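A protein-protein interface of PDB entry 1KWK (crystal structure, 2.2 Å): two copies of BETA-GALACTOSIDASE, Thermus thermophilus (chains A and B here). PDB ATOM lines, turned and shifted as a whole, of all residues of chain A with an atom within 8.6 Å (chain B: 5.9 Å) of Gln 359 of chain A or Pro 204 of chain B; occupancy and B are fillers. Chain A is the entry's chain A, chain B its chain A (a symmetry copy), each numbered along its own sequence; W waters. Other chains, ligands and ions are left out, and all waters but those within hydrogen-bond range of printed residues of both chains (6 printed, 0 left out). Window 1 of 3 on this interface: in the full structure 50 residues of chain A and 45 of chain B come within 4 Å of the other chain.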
ATOM      1  N   PHE A  99      -5.216  21.527  28.735  1.00  0.00           N
ATOM      2  CA  PHE A  99      -3.804  21.865  28.822  1.00  0.00           C
ATOM      3  C   PHE A  99      -3.352  22.022  27.369  1.00  0.00           C
ATOM      4  O   PHE A  99      -4.027  21.534  26.463  1.00  0.00           O
ATOM      5  CB  PHE A  99      -3.068  20.708  29.511  1.00  0.00           C
ATOM      6  CG  PHE A  99      -1.595  20.932  29.705  1.00  0.00           C
ATOM      7  CD1 PHE A  99      -0.678  20.493  28.757  1.00  0.00           C
ATOM      8  CD2 PHE A  99      -1.121  21.553  30.856  1.00  0.00           C
ATOM      9  CE1 PHE A  99       0.692  20.665  28.955  1.00  0.00           C
ATOM     10  CE2 PHE A  99       0.245  21.731  31.064  1.00  0.00           C
ATOM     11  CZ  PHE A  99       1.152  21.285  30.111  1.00  0.00           C
ATOM     12  N   GLY A 100      -2.235  22.709  27.142  1.00  0.00           N
ATOM     13  CA  GLY A 100      -1.757  22.884  25.778  1.00  0.00           C
ATOM     14  C   GLY A 100      -1.291  24.297  25.472  1.00  0.00           C
ATOM     15  O   GLY A 100      -0.426  24.505  24.621  1.00  0.00           O
ATOM     16  N   GLY A 101      -1.878  25.268  26.161  1.00  0.00           N
ATOM     17  CA  GLY A 101      -1.500  26.654  25.969  1.00  0.00           C
ATOM     18  C   GLY A 101      -0.997  27.209  27.287  1.00  0.00           C
ATOM     19  O   GLY A 101       0.069  26.813  27.769  1.00  0.00           O
ATOM     20  N   ARG A 102      -1.768  28.122  27.869  1.00  0.00           N
ATOM     21  CA  ARG A 102      -1.422  28.729  29.150  1.00  0.00           C
ATOM     22  C   ARG A 102      -2.678  29.245  29.852  1.00  0.00           C
ATOM     23  O   ARG A 102      -3.771  29.223  29.285  1.00  0.00           O
ATOM     24  CB  ARG A 102      -0.436  29.885  28.951  1.00  0.00           C
ATOM     25  CG  ARG A 102      -0.985  31.066  28.165  1.00  0.00           C
ATOM     26  CD  ARG A 102       0.035  32.187  28.131  1.00  0.00           C
ATOM     27  NE  ARG A 102      -0.331  33.233  27.186  1.00  0.00           N
ATOM     28  CZ  ARG A 102       0.464  34.242  26.844  1.00  0.00           C
ATOM     29  NH1 ARG A 102       1.677  34.345  27.377  1.00  0.00           N
ATOM     30  NH2 ARG A 102       0.051  35.139  25.955  1.00  0.00           N
ATOM     31  N   HIS A 104      -4.506  27.978  31.947  1.00  0.00           N
ATOM     32  CA  HIS A 104      -5.545  26.959  32.058  1.00  0.00           C
ATOM     33  C   HIS A 104      -5.835  26.588  33.512  1.00  0.00           C
ATOM     34  O   HIS A 104      -5.636  25.441  33.925  1.00  0.00           O
ATOM     35  CB  HIS A 104      -5.148  25.699  31.278  1.00  0.00           C
ATOM     36  CG  HIS A 104      -3.713  25.313  31.450  1.00  0.00           C
ATOM     37  ND1 HIS A 104      -2.719  25.756  30.606  1.00  0.00           N
ATOM     38  CD2 HIS A 104      -3.099  24.564  32.396  1.00  0.00           C
ATOM     39  CE1 HIS A 104      -1.553  25.298  31.025  1.00  0.00           C
ATOM     40  NE2 HIS A 104      -1.755  24.572  32.110  1.00  0.00           N
ATOM     41  N   HIS A 145      -6.713  35.918  27.675  1.00  0.00           N
ATOM     42  CA  HIS A 145      -7.496  34.870  27.021  1.00  0.00           C
ATOM     43  C   HIS A 145      -8.847  34.694  27.718  1.00  0.00           C
ATOM     44  O   HIS A 145      -9.356  33.578  27.832  1.00  0.00           O
ATOM     45  CB  HIS A 145      -6.729  33.539  27.016  1.00  0.00           C
ATOM     46  CG  HIS A 145      -5.383  33.618  26.361  1.00  0.00           C
ATOM     47  ND1 HIS A 145      -5.212  34.034  25.057  1.00  0.00           N
ATOM     48  CD2 HIS A 145      -4.145  33.338  26.832  1.00  0.00           C
ATOM     49  CE1 HIS A 145      -3.926  34.007  24.754  1.00  0.00           C
ATOM     50  NE2 HIS A 145      -3.257  33.588  25.813  1.00  0.00           N
ATOM     51  N   VAL A 318       4.620  40.962  16.369  1.00  0.00           N
ATOM     52  CA  VAL A 318       4.096  39.961  17.295  1.00  0.00           C
ATOM     53  C   VAL A 318       3.459  38.841  16.481  1.00  0.00           C
ATOM     54  O   VAL A 318       3.510  38.845  15.248  1.00  0.00           O
ATOM     55  CB  VAL A 318       3.036  40.550  18.280  1.00  0.00           C
ATOM     56  CG1 VAL A 318       3.682  41.584  19.179  1.00  0.00           C
ATOM     57  CG2 VAL A 318       1.871  41.160  17.509  1.00  0.00           C
ATOM     58  N   ASN A 319       2.833  37.896  17.169  1.00  0.00           N
ATOM     59  CA  ASN A 319       2.239  36.740  16.504  1.00  0.00           C
ATOM     60  C   ASN A 319       0.731  36.582  16.629  1.00  0.00           C
ATOM     61  O   ASN A 319       0.123  35.808  15.880  1.00  0.00           O
ATOM     62  CB  ASN A 319       2.847  35.480  17.099  1.00  0.00           C
ATOM     63  CG  ASN A 319       2.510  35.337  18.576  1.00  0.00           C
ATOM     64  OD1 ASN A 319       3.046  36.061  19.420  1.00  0.00           O
ATOM     65  ND2 ASN A 319       1.592  34.428  18.890  1.00  0.00           N
ATOM     66  N   TRP A 320       0.127  37.305  17.562  1.00  0.00           N
ATOM     67  CA  TRP A 320      -1.291  37.115  17.853  1.00  0.00           C
ATOM     68  C   TRP A 320      -2.409  37.964  17.250  1.00  0.00           C
ATOM     69  O   TRP A 320      -3.582  37.666  17.474  1.00  0.00           O
ATOM     70  CB  TRP A 320      -1.458  37.106  19.371  1.00  0.00           C
ATOM     71  CG  TRP A 320      -0.764  38.258  20.041  1.00  0.00           C
ATOM     72  CD1 TRP A 320       0.479  38.251  20.614  1.00  0.00           C
ATOM     73  CD2 TRP A 320      -1.274  39.588  20.207  1.00  0.00           C
ATOM     74  NE1 TRP A 320       0.771  39.493  21.129  1.00  0.00           N
ATOM     75  CE2 TRP A 320      -0.285  40.333  20.893  1.00  0.00           C
ATOM     76  CE3 TRP A 320      -2.471  40.224  19.843  1.00  0.00           C
ATOM     77  CZ2 TRP A 320      -0.459  41.682  21.226  1.00  0.00           C
ATOM     78  CZ3 TRP A 320      -2.645  41.568  20.176  1.00  0.00           C
ATOM     79  CH2 TRP A 320      -1.641  42.280  20.860  1.00  0.00           C
ATOM     80  N   ALA A 355      12.033  32.998  19.948  1.00  0.00           N
ATOM     81  CA  ALA A 355      12.021  31.550  20.118  1.00  0.00           C
ATOM     82  C   ALA A 355      11.763  30.884  18.765  1.00  0.00           C
ATOM     83  O   ALA A 355      10.887  31.307  18.011  1.00  0.00           O
ATOM     84  CB  ALA A 355      10.943  31.147  21.112  1.00  0.00           C
ATOM     85  N   PRO A 356      12.531  29.832  18.439  1.00  0.00           N
ATOM     86  CA  PRO A 356      12.350  29.136  17.162  1.00  0.00           C
ATOM     87  C   PRO A 356      11.295  28.027  17.212  1.00  0.00           C
ATOM     88  O   PRO A 356      11.043  27.359  16.213  1.00  0.00           O
ATOM     89  CB  PRO A 356      13.749  28.595  16.879  1.00  0.00           C
ATOM     90  CG  PRO A 356      14.215  28.202  18.248  1.00  0.00           C
ATOM     91  CD  PRO A 356      13.751  29.364  19.127  1.00  0.00           C
ATOM     92  N   PHE A 357      10.672  27.842  18.369  1.00  0.00           N
ATOM     93  CA  PHE A 357       9.666  26.796  18.527  1.00  0.00           C
ATOM     94  C   PHE A 357       8.428  27.255  19.302  1.00  0.00           C
ATOM     95  O   PHE A 357       8.410  28.342  19.884  1.00  0.00           O
ATOM     96  CB  PHE A 357      10.291  25.594  19.246  1.00  0.00           C
ATOM     97  CG  PHE A 357      11.057  25.969  20.488  1.00  0.00           C
ATOM     98  CD1 PHE A 357      12.449  25.945  20.498  1.00  0.00           C
ATOM     99  CD2 PHE A 357      10.386  26.398  21.632  1.00  0.00           C
ATOM    100  CE1 PHE A 357      13.164  26.348  21.634  1.00  0.00           C
ATOM    101  CE2 PHE A 357      11.086  26.803  22.767  1.00  0.00           C
ATOM    102  CZ  PHE A 357      12.479  26.778  22.768  1.00  0.00           C
ATOM    103  N   ALA A 358       7.401  26.408  19.299  1.00  0.00           N
ATOM    104  CA  ALA A 358       6.157  26.671  20.018  1.00  0.00           C
ATOM    105  C   ALA A 358       5.283  27.794  19.458  1.00  0.00           C
ATOM    106  O   ALA A 358       5.563  28.349  18.393  1.00  0.00           O
ATOM    107  CB  ALA A 358       6.458  26.924  21.496  1.00  0.00           C
ATOM    108  N   GLN A 359       4.228  28.116  20.207  1.00  0.00           N
ATOM    109  CA  GLN A 359       3.230  29.121  19.836  1.00  0.00           C
ATOM    110  C   GLN A 359       3.691  30.502  19.389  1.00  0.00           C
ATOM    111  O   GLN A 359       3.127  31.068  18.450  1.00  0.00           O
ATOM    112  CB  GLN A 359       2.223  29.308  20.978  1.00  0.00           C
ATOM    113  CG  GLN A 359       1.294  28.124  21.186  1.00  0.00           C
ATOM    114  CD  GLN A 359       1.805  27.137  22.218  1.00  0.00           C
ATOM    115  OE1 GLN A 359       3.014  26.910  22.349  1.00  0.00           O
ATOM    116  NE2 GLN A 359       0.878  26.531  22.951  1.00  0.00           N
ATOM    117  N   GLU A 360       4.700  31.052  20.056  1.00  0.00           N
ATOM    118  CA  GLU A 360       5.169  32.385  19.708  1.00  0.00           C
ATOM    119  C   GLU A 360       6.472  32.424  18.931  1.00  0.00           C
ATOM    120  O   GLU A 360       7.266  33.358  19.073  1.00  0.00           O
ATOM    121  CB  GLU A 360       5.272  33.233  20.980  1.00  0.00           C
ATOM    122  CG  GLU A 360       3.915  33.432  21.643  1.00  0.00           C
ATOM    123  CD  GLU A 360       3.975  34.252  22.911  1.00  0.00           C
ATOM    124  OE1 GLU A 360       2.902  34.725  23.339  1.00  0.00           O
ATOM    125  OE2 GLU A 360       5.076  34.416  23.483  1.00  0.00           O
ATOM    126  N   GLN A 361       6.693  31.417  18.092  1.00  0.00           N
ATOM    127  CA  GLN A 361       7.911  31.389  17.301  1.00  0.00           C
ATOM    128  C   GLN A 361       7.944  32.569  16.323  1.00  0.00           C
ATOM    129  O   GLN A 361       9.012  32.966  15.868  1.00  0.00           O
ATOM    130  CB  GLN A 361       8.032  30.060  16.545  1.00  0.00           C
ATOM    131  CG  GLN A 361       6.960  29.807  15.491  1.00  0.00           C
ATOM    132  CD  GLN A 361       7.071  28.414  14.894  1.00  0.00           C
ATOM    133  OE1 GLN A 361       7.270  28.250  13.687  1.00  0.00           O
ATOM    134  NE2 GLN A 361       6.942  27.397  15.744  1.00  0.00           N
ATOM    135  N   MET A 362       6.785  33.139  16.001  1.00  0.00           N
ATOM    136  CA  MET A 362       6.755  34.282  15.090  1.00  0.00           C
ATOM    137  C   MET A 362       6.808  35.619  15.849  1.00  0.00           C
ATOM    138  O   MET A 362       6.738  36.686  15.236  1.00  0.00           O
ATOM    139  CB  MET A 362       5.507  34.239  14.201  1.00  0.00           C
ATOM    140  CG  MET A 362       5.421  32.990  13.330  1.00  0.00           C
ATOM    141  SD  MET A 362       6.867  32.775  12.259  1.00  0.00           S
ATOM    142  CE  MET A 362       6.294  33.557  10.746  1.00  0.00           C
ATOM    143  N   HIS A 363       6.934  35.561  17.174  1.00  0.00           N
ATOM    144  CA  HIS A 363       7.011  36.785  17.983  1.00  0.00           C
ATOM    145  C   HIS A 363       8.475  37.208  18.064  1.00  0.00           C
ATOM    146  O   HIS A 363       9.303  36.512  18.658  1.00  0.00           O
ATOM    147  CB  HIS A 363       6.461  36.546  19.393  1.00  0.00           C
ATOM    148  CG  HIS A 363       6.292  37.798  20.199  1.00  0.00           C
ATOM    149  ND1 HIS A 363       7.332  38.671  20.455  1.00  0.00           N
ATOM    150  CD2 HIS A 363       5.206  38.317  20.819  1.00  0.00           C
ATOM    151  CE1 HIS A 363       6.893  39.670  21.199  1.00  0.00           C
ATOM    152  NE2 HIS A 363       5.606  39.480  21.435  1.00  0.00           N
ATOM    153  N   PHE B 181       8.467  25.767  26.561  1.00  0.00           N
ATOM    154  CA  PHE B 181       7.626  26.952  26.391  1.00  0.00           C
ATOM    155  C   PHE B 181       6.266  26.806  27.083  1.00  0.00           C
ATOM    156  O   PHE B 181       5.545  25.829  26.859  1.00  0.00           O
ATOM    157  CB  PHE B 181       7.437  27.217  24.889  1.00  0.00           C
ATOM    158  CG  PHE B 181       6.763  28.525  24.572  1.00  0.00           C
ATOM    159  CD1 PHE B 181       5.405  28.571  24.280  1.00  0.00           C
ATOM    160  CD2 PHE B 181       7.495  29.711  24.547  1.00  0.00           C
ATOM    161  CE1 PHE B 181       4.782  29.779  23.963  1.00  0.00           C
ATOM    162  CE2 PHE B 181       6.885  30.924  24.234  1.00  0.00           C
ATOM    163  CZ  PHE B 181       5.524  30.958  23.940  1.00  0.00           C
ATOM    164  N   TRP B 182       5.921  27.792  27.911  1.00  0.00           N
ATOM    165  CA  TRP B 182       4.662  27.791  28.662  1.00  0.00           C
ATOM    166  C   TRP B 182       4.483  26.519  29.493  1.00  0.00           C
ATOM    167  O   TRP B 182       3.363  26.039  29.660  1.00  0.00           O
ATOM    168  CB  TRP B 182       3.459  27.950  27.720  1.00  0.00           C
ATOM    169  CG  TRP B 182       3.304  29.327  27.119  1.00  0.00           C
ATOM    170  CD1 TRP B 182       4.016  30.456  27.435  1.00  0.00           C
ATOM    171  CD2 TRP B 182       2.353  29.719  26.119  1.00  0.00           C
ATOM    172  NE1 TRP B 182       3.560  31.523  26.693  1.00  0.00           N
ATOM    173  CE2 TRP B 182       2.542  31.098  25.878  1.00  0.00           C
ATOM    174  CE3 TRP B 182       1.357  29.035  25.401  1.00  0.00           C
ATOM    175  CZ2 TRP B 182       1.772  31.809  24.949  1.00  0.00           C
ATOM    176  CZ3 TRP B 182       0.591  29.743  24.477  1.00  0.00           C
ATOM    177  CH2 TRP B 182       0.805  31.116  24.261  1.00  0.00           C
ATOM    178  N   GLN B 184       4.856  23.348  28.993  1.00  0.00           N
ATOM    179  CA  GLN B 184       4.056  22.321  28.335  1.00  0.00           C
ATOM    180  C   GLN B 184       4.682  20.931  28.471  1.00  0.00           C
ATOM    181  O   GLN B 184       4.078  19.936  28.074  1.00  0.00           O
ATOM    182  CB  GLN B 184       3.903  22.651  26.848  1.00  0.00           C
ATOM    183  CG  GLN B 184       3.129  23.923  26.556  1.00  0.00           C
ATOM    184  CD  GLN B 184       3.122  24.263  25.075  1.00  0.00           C
ATOM    185  OE1 GLN B 184       2.691  23.463  24.244  1.00  0.00           O
ATOM    186  NE2 GLN B 184       3.606  25.453  24.741  1.00  0.00           N
ATOM    187  N   GLU B 201      -3.639  29.667  22.310  1.00  0.00           N
ATOM    188  CA  GLU B 201      -3.411  28.821  21.146  1.00  0.00           C
ATOM    189  C   GLU B 201      -2.646  27.534  21.458  1.00  0.00           C
ATOM    190  O   GLU B 201      -1.783  27.505  22.338  1.00  0.00           O
ATOM    191  CB  GLU B 201      -2.675  29.612  20.059  1.00  0.00           C
ATOM    192  CG  GLU B 201      -3.435  30.840  19.548  1.00  0.00           C
ATOM    193  CD  GLU B 201      -3.205  32.097  20.392  1.00  0.00           C
ATOM    194  OE1 GLU B 201      -3.365  32.041  21.632  1.00  0.00           O
ATOM    195  OE2 GLU B 201      -2.870  33.151  19.806  1.00  0.00           O
ATOM    196  N   PRO B 202      -2.979  26.442  20.754  1.00  0.00           N
ATOM    197  CA  PRO B 202      -2.297  25.161  20.971  1.00  0.00           C
ATOM    198  C   PRO B 202      -0.912  25.231  20.324  1.00  0.00           C
ATOM    199  O   PRO B 202      -0.651  26.119  19.506  1.00  0.00           O
ATOM    200  CB  PRO B 202      -3.216  24.160  20.278  1.00  0.00           C
ATOM    201  CG  PRO B 202      -3.756  24.963  19.125  1.00  0.00           C
ATOM    202  CD  PRO B 202      -4.076  26.297  19.780  1.00  0.00           C
ATOM    203  N   ASN B 203      -0.031  24.307  20.688  1.00  0.00           N
ATOM    204  CA  ASN B 203       1.316  24.292  20.134  1.00  0.00           C
ATOM    205  C   ASN B 203       1.248  23.926  18.653  1.00  0.00           C
ATOM    206  O   ASN B 203       0.628  22.930  18.286  1.00  0.00           O
ATOM    207  CB  ASN B 203       2.184  23.279  20.887  1.00  0.00           C
ATOM    208  CG  ASN B 203       3.650  23.365  20.498  1.00  0.00           C
ATOM    209  OD1 ASN B 203       3.995  23.357  19.315  1.00  0.00           O
ATOM    210  ND2 ASN B 203       4.524  23.443  21.497  1.00  0.00           N
ATOM    211  N   PRO B 204       1.881  24.727  17.780  1.00  0.00           N
ATOM    212  CA  PRO B 204       1.859  24.448  16.340  1.00  0.00           C
ATOM    213  C   PRO B 204       2.401  23.081  15.927  1.00  0.00           C
ATOM    214  O   PRO B 204       1.857  22.451  15.018  1.00  0.00           O
ATOM    215  CB  PRO B 204       2.661  25.615  15.745  1.00  0.00           C
ATOM    216  CG  PRO B 204       3.578  26.009  16.856  1.00  0.00           C
ATOM    217  CD  PRO B 204       2.684  25.928  18.066  1.00  0.00           C
ATOM    218  N   SER B 205       3.464  22.623  16.586  1.00  0.00           N
ATOM    219  CA  SER B 205       4.047  21.320  16.270  1.00  0.00           C
ATOM    220  C   SER B 205       3.059  20.243  16.675  1.00  0.00           C
ATOM    221  O   SER B 205       2.900  19.238  15.990  1.00  0.00           O
ATOM    222  CB  SER B 205       5.354  21.101  17.037  1.00  0.00           C
ATOM    223  OG  SER B 205       6.230  22.195  16.863  1.00  0.00           O
ATOM    224  N   HIS B 206       2.406  20.477  17.807  1.00  0.00           N
ATOM    225  CA  HIS B 206       1.416  19.566  18.369  1.00  0.00           C
ATOM    226  C   HIS B 206       0.225  19.471  17.419  1.00  0.00           C
ATOM    227  O   HIS B 206      -0.231  18.377  17.079  1.00  0.00           O
ATOM    228  CB  HIS B 206       0.973  20.105  19.740  1.00  0.00           C
ATOM    229  CG  HIS B 206      -0.057  19.265  20.436  1.00  0.00           C
ATOM    230  ND1 HIS B 206      -0.596  19.618  21.656  1.00  0.00           N
ATOM    231  CD2 HIS B 206      -0.642  18.093  20.092  1.00  0.00           C
ATOM    232  CE1 HIS B 206      -1.468  18.699  22.032  1.00  0.00           C
ATOM    233  NE2 HIS B 206      -1.516  17.763  21.101  1.00  0.00           N
ATOM    234  N   LEU B 207      -0.269  20.627  16.985  1.00  0.00           N
ATOM    235  CA  LEU B 207      -1.410  20.676  16.084  1.00  0.00           C
ATOM    236  C   LEU B 207      -1.091  20.107  14.704  1.00  0.00           C
ATOM    237  O   LEU B 207      -1.942  19.466  14.085  1.00  0.00           O
ATOM    238  CB  LEU B 207      -1.905  22.116  15.953  1.00  0.00           C
ATOM    239  CG  LEU B 207      -3.237  22.339  15.245  1.00  0.00           C
ATOM    240  CD1 LEU B 207      -4.325  21.536  15.935  1.00  0.00           C
ATOM    241  CD2 LEU B 207      -3.582  23.829  15.266  1.00  0.00           C
ATOM    242  N   LEU B 208       0.131  20.329  14.225  1.00  0.00           N
ATOM    243  CA  LEU B 208       0.523  19.813  12.915  1.00  0.00           C
ATOM    244  C   LEU B 208       0.586  18.290  12.936  1.00  0.00           C
ATOM    245  O   LEU B 208       0.108  17.637  12.010  1.00  0.00           O
ATOM    246  CB  LEU B 208       1.879  20.379  12.478  1.00  0.00           C
ATOM    247  CG  LEU B 208       2.491  19.725  11.229  1.00  0.00           C
ATOM    248  CD1 LEU B 208       1.537  19.863  10.050  1.00  0.00           C
ATOM    249  CD2 LEU B 208       3.826  20.367  10.910  1.00  0.00           C
ATOM    250  N   ASP B 209       1.178  17.725  13.989  1.00  0.00           N
ATOM    251  CA  ASP B 209       1.272  16.271  14.101  1.00  0.00           C
ATOM    252  C   ASP B 209      -0.123  15.670  14.176  1.00  0.00           C
ATOM    253  O   ASP B 209      -0.356  14.557  13.711  1.00  0.00           O
ATOM    254  CB  ASP B 209       2.071  15.856  15.343  1.00  0.00           C
ATOM    255  CG  ASP B 209       3.571  15.885  15.110  1.00  0.00           C
ATOM    256  OD1 ASP B 209       3.997  15.913  13.935  1.00  0.00           O
ATOM    257  OD2 ASP B 209       4.326  15.861  16.102  1.00  0.00           O
ATOM    258  N   VAL B 414      -2.324  25.941  10.520  1.00  0.00           N
ATOM    259  CA  VAL B 414      -1.905  26.018  11.916  1.00  0.00           C
ATOM    260  C   VAL B 414      -1.336  27.387  12.289  1.00  0.00           C
ATOM    261  O   VAL B 414      -1.542  27.875  13.399  1.00  0.00           O
ATOM    262  CB  VAL B 414      -0.816  24.961  12.224  1.00  0.00           C
ATOM    263  CG1 VAL B 414      -0.274  25.152  13.643  1.00  0.00           C
ATOM    264  CG2 VAL B 414      -1.389  23.562  12.055  1.00  0.00           C
ATOM    265  N   GLN B 415      -0.630  28.008  11.355  1.00  0.00           N
ATOM    266  CA  GLN B 415      -0.004  29.291  11.621  1.00  0.00           C
ATOM    267  C   GLN B 415      -0.095  30.246  10.433  1.00  0.00           C
ATOM    268  O   GLN B 415       0.874  30.425   9.691  1.00  0.00           O
ATOM    269  CB  GLN B 415       1.472  29.056  11.978  1.00  0.00           C
ATOM    270  CG  GLN B 415       2.221  30.291  12.452  1.00  0.00           C
ATOM    271  CD  GLN B 415       3.720  30.073  12.482  1.00  0.00           C
ATOM    272  OE1 GLN B 415       4.425  30.367  11.510  1.00  0.00           O
ATOM    273  NE2 GLN B 415       4.216  29.536  13.590  1.00  0.00           N
ATOM    274  N   PHE B 492       8.099  21.742  12.893  1.00  0.00           N
ATOM    275  CA  PHE B 492       7.465  23.044  13.004  1.00  0.00           C
ATOM    276  C   PHE B 492       8.276  24.023  13.849  1.00  0.00           C
ATOM    277  O   PHE B 492       7.760  24.658  14.773  1.00  0.00           O
ATOM    278  CB  PHE B 492       6.049  22.883  13.575  1.00  0.00           C
ATOM    279  CG  PHE B 492       5.046  23.851  13.002  1.00  0.00           C
ATOM    280  CD1 PHE B 492       3.768  23.416  12.648  1.00  0.00           C
ATOM    281  CD2 PHE B 492       5.368  25.196  12.826  1.00  0.00           C
ATOM    282  CE1 PHE B 492       2.822  24.308  12.124  1.00  0.00           C
ATOM    283  CE2 PHE B 492       4.431  26.095  12.305  1.00  0.00           C
ATOM    284  CZ  PHE B 492       3.154  25.648  11.954  1.00  0.00           C
HETATM  285  O   HOH W   1      -4.166  35.261  18.644  1.00  0.00           O
HETATM  286  O   HOH W   2      -0.714  22.547  22.554  1.00  0.00           O
HETATM  287  O   HOH W   3       5.328  33.862  26.357  1.00  0.00           O
HETATM  288  O   HOH W   4       7.874  24.035  17.557  1.00  0.00           O
HETATM  289  O   HOH W   5       2.481  29.297  15.748  1.00  0.00           O
HETATM  290  O   HOH W   6       1.440  24.702  30.838  1.00  0.00           O
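Phe 357 of chain A touches none of the printed residues of chain B. Gln 359 of chain A touches just these residues of chain B: Phe 181 (3.5 Å), Trp 182 (3.5 Å), Gln 184 (2.9 Å), Glu 201 (2.9 Å), Pro 202 (3.3 Å), Asn 203 (3.3 Å) and Pro 204 (3.4 Å). Of the printed residues of chain B, Met 362 of chain A touches Gln 415. Printed residues of chain A within 4 Å of Gln 184 of chain B: Phe 99, Gly 100 and Gln 359. Of the printed residues of chain A, Glu 201 of chain B touches Gly 101, His 145 and Gln 359. Of the printed residues of chain A, Asn 203 of chain B touches Gly 100, Ala 358 and Gln 359. Pro 204 of chain B touches three residues of chain A. No residue of chain A comes within 4 Å of Ser 205 of chain B. The nearest residue of chain B that does not touch Gln 359 of chain A is Gln 415 of chain B (5.2 Å).
Hydrophobic or aromatic side chains of chain B within 4 Å of the printed part of chain A: Phe 181, Trp 182, Pro 204 and Phe 492. Of the 18 printed residues of chain A, 10 touch a printed residue of chain B. Among the printed residues, 23 pairs touch across the chains.
Gln 184 of chain B touches Phe 99 of chain A (CA to CZ, 3.6 Å). Gly 100 of chain A touches Asn 203 of chain B (O to N, 3.96 Å). O of Gly 101 of chain A touches CE3 of Trp 182 of chain B, 3.5 Å away. Glu 201 of chain B touches Gly 101 of chain A (O to CA, 3.7 Å). Ala 358 of chain A touches Phe 181 of chain B (CB to CD1, 3.4 Å). Asn 203 of chain B touches Ala 358 of chain A (ND2 to CA, 3.9 Å). Pro 204 of chain B touches Ala 358 of chain A. N of Gln 359 of chain A touches CD of Pro 204 of chain B (3.4 Å). Glu 360 of chain A touches Phe 181 of chain B. Glu 360 of chain A touches Trp 182 of chain B.
The side-chain amide nitrogen of Gln 359 of chain A lies within hydrogen-bond range of the backbone carbonyl oxygen of Gly 100 of chain A (2.9 Å). The guanidinium group (NH2) of Arg 102 of chain A is in salt-bridge range of the side-chain carboxylate (OE1) of Glu 360 of chain A. The side-chain amide nitrogen (NE2) of Gln 361 of chain A sits at hydrogen-bond distance from the backbone carbonyl oxygen (O) of Ala 358 of chain A, at 3.1 Å. O of Phe 181 of chain B is in hydrogen-bond range of NE2 of Gln 184 of chain B (2.9 Å). The side-chain amide oxygen (OE1) of Gln 184 of chain B lies within hydrogen-bond range of the side-chain amide nitrogen (ND2) of Asn 203 of chain B (3.3 Å). The side-chain amide oxygen (OD1) of Asn 203 of chain B sits at hydrogen-bond distance from the backbone NH (N) of Ser 205 of chain B (2.9 Å).
Water W4 lies within hydrogen-bond range of the side-chain hydroxyl (OG) of Ser 205 of chain B, the backbone carbonyl oxygen (O) of Phe 492 of chain B and the backbone NH (N) of Ala 358 of chain A. Water W2 lies within hydrogen-bond range of N of Asn 203 of chain B, O of Gly 100 of chain A and ND1 of His 206 of chain B. Water W1 lies within hydrogen-bond range of the side-chain carboxylate of Glu 201 of chain B (2.7 Å) and the backbone carbonyl oxygen of Trp 320 of chain A (2.7 Å). Water W5 bridges the side-chain amide nitrogen (NE2) of Gln 415 of chain B (2.8 Å) and the backbone carbonyl oxygen (O) of Gln 359 of chain A (3.3 Å). Water W3 lies within hydrogen-bond range of OE2 of Glu 360 of chain A (2.9 Å) and NE1 of Trp 182 of chain B (3.0 Å).
No position is printed for both chains. Of the 23 pairs that touch across the chains among the printed residues, none has its exchanged pair printed and touching as well.
O of Gly 100 of chain A sits close to OE1 of Gln 184 of chain B, at 3.3 Å. The side-chain amide oxygen of Gln 359 of chain A lies within hydrogen-bond range of the side-chain amide nitrogen of Gln 184 of chain B. The backbone carbonyl oxygen (O) of Glu 201 of chain B is in hydrogen-bond range of the side-chain amide nitrogen (NE2) of Gln 359 of chain A, at 2.9 Å. NE2 of Gln 359 of chain A sits close to N of Asn 203 of chain B (3.3 Å). The side-chain amide oxygen of Gln 361 of chain A is in hydrogen-bond range of the side-chain amide nitrogen of Gln 415 of chain B, at 3.3 Å. The backbone carbonyl oxygen of Phe 492 of chain B sits at hydrogen-bond distance from the side-chain amide nitrogen of Gln 361 of chain A (3.0 Å). The side-chain sulfur of Met 362 of chain A sits close to the side-chain amide oxygen of Gln 415 of chain B. The guanidinium group (NH1) of Arg 102 of chain A lies close to the indole nitrogen (NE1) of Trp 182 of chain B (3.5 Å).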
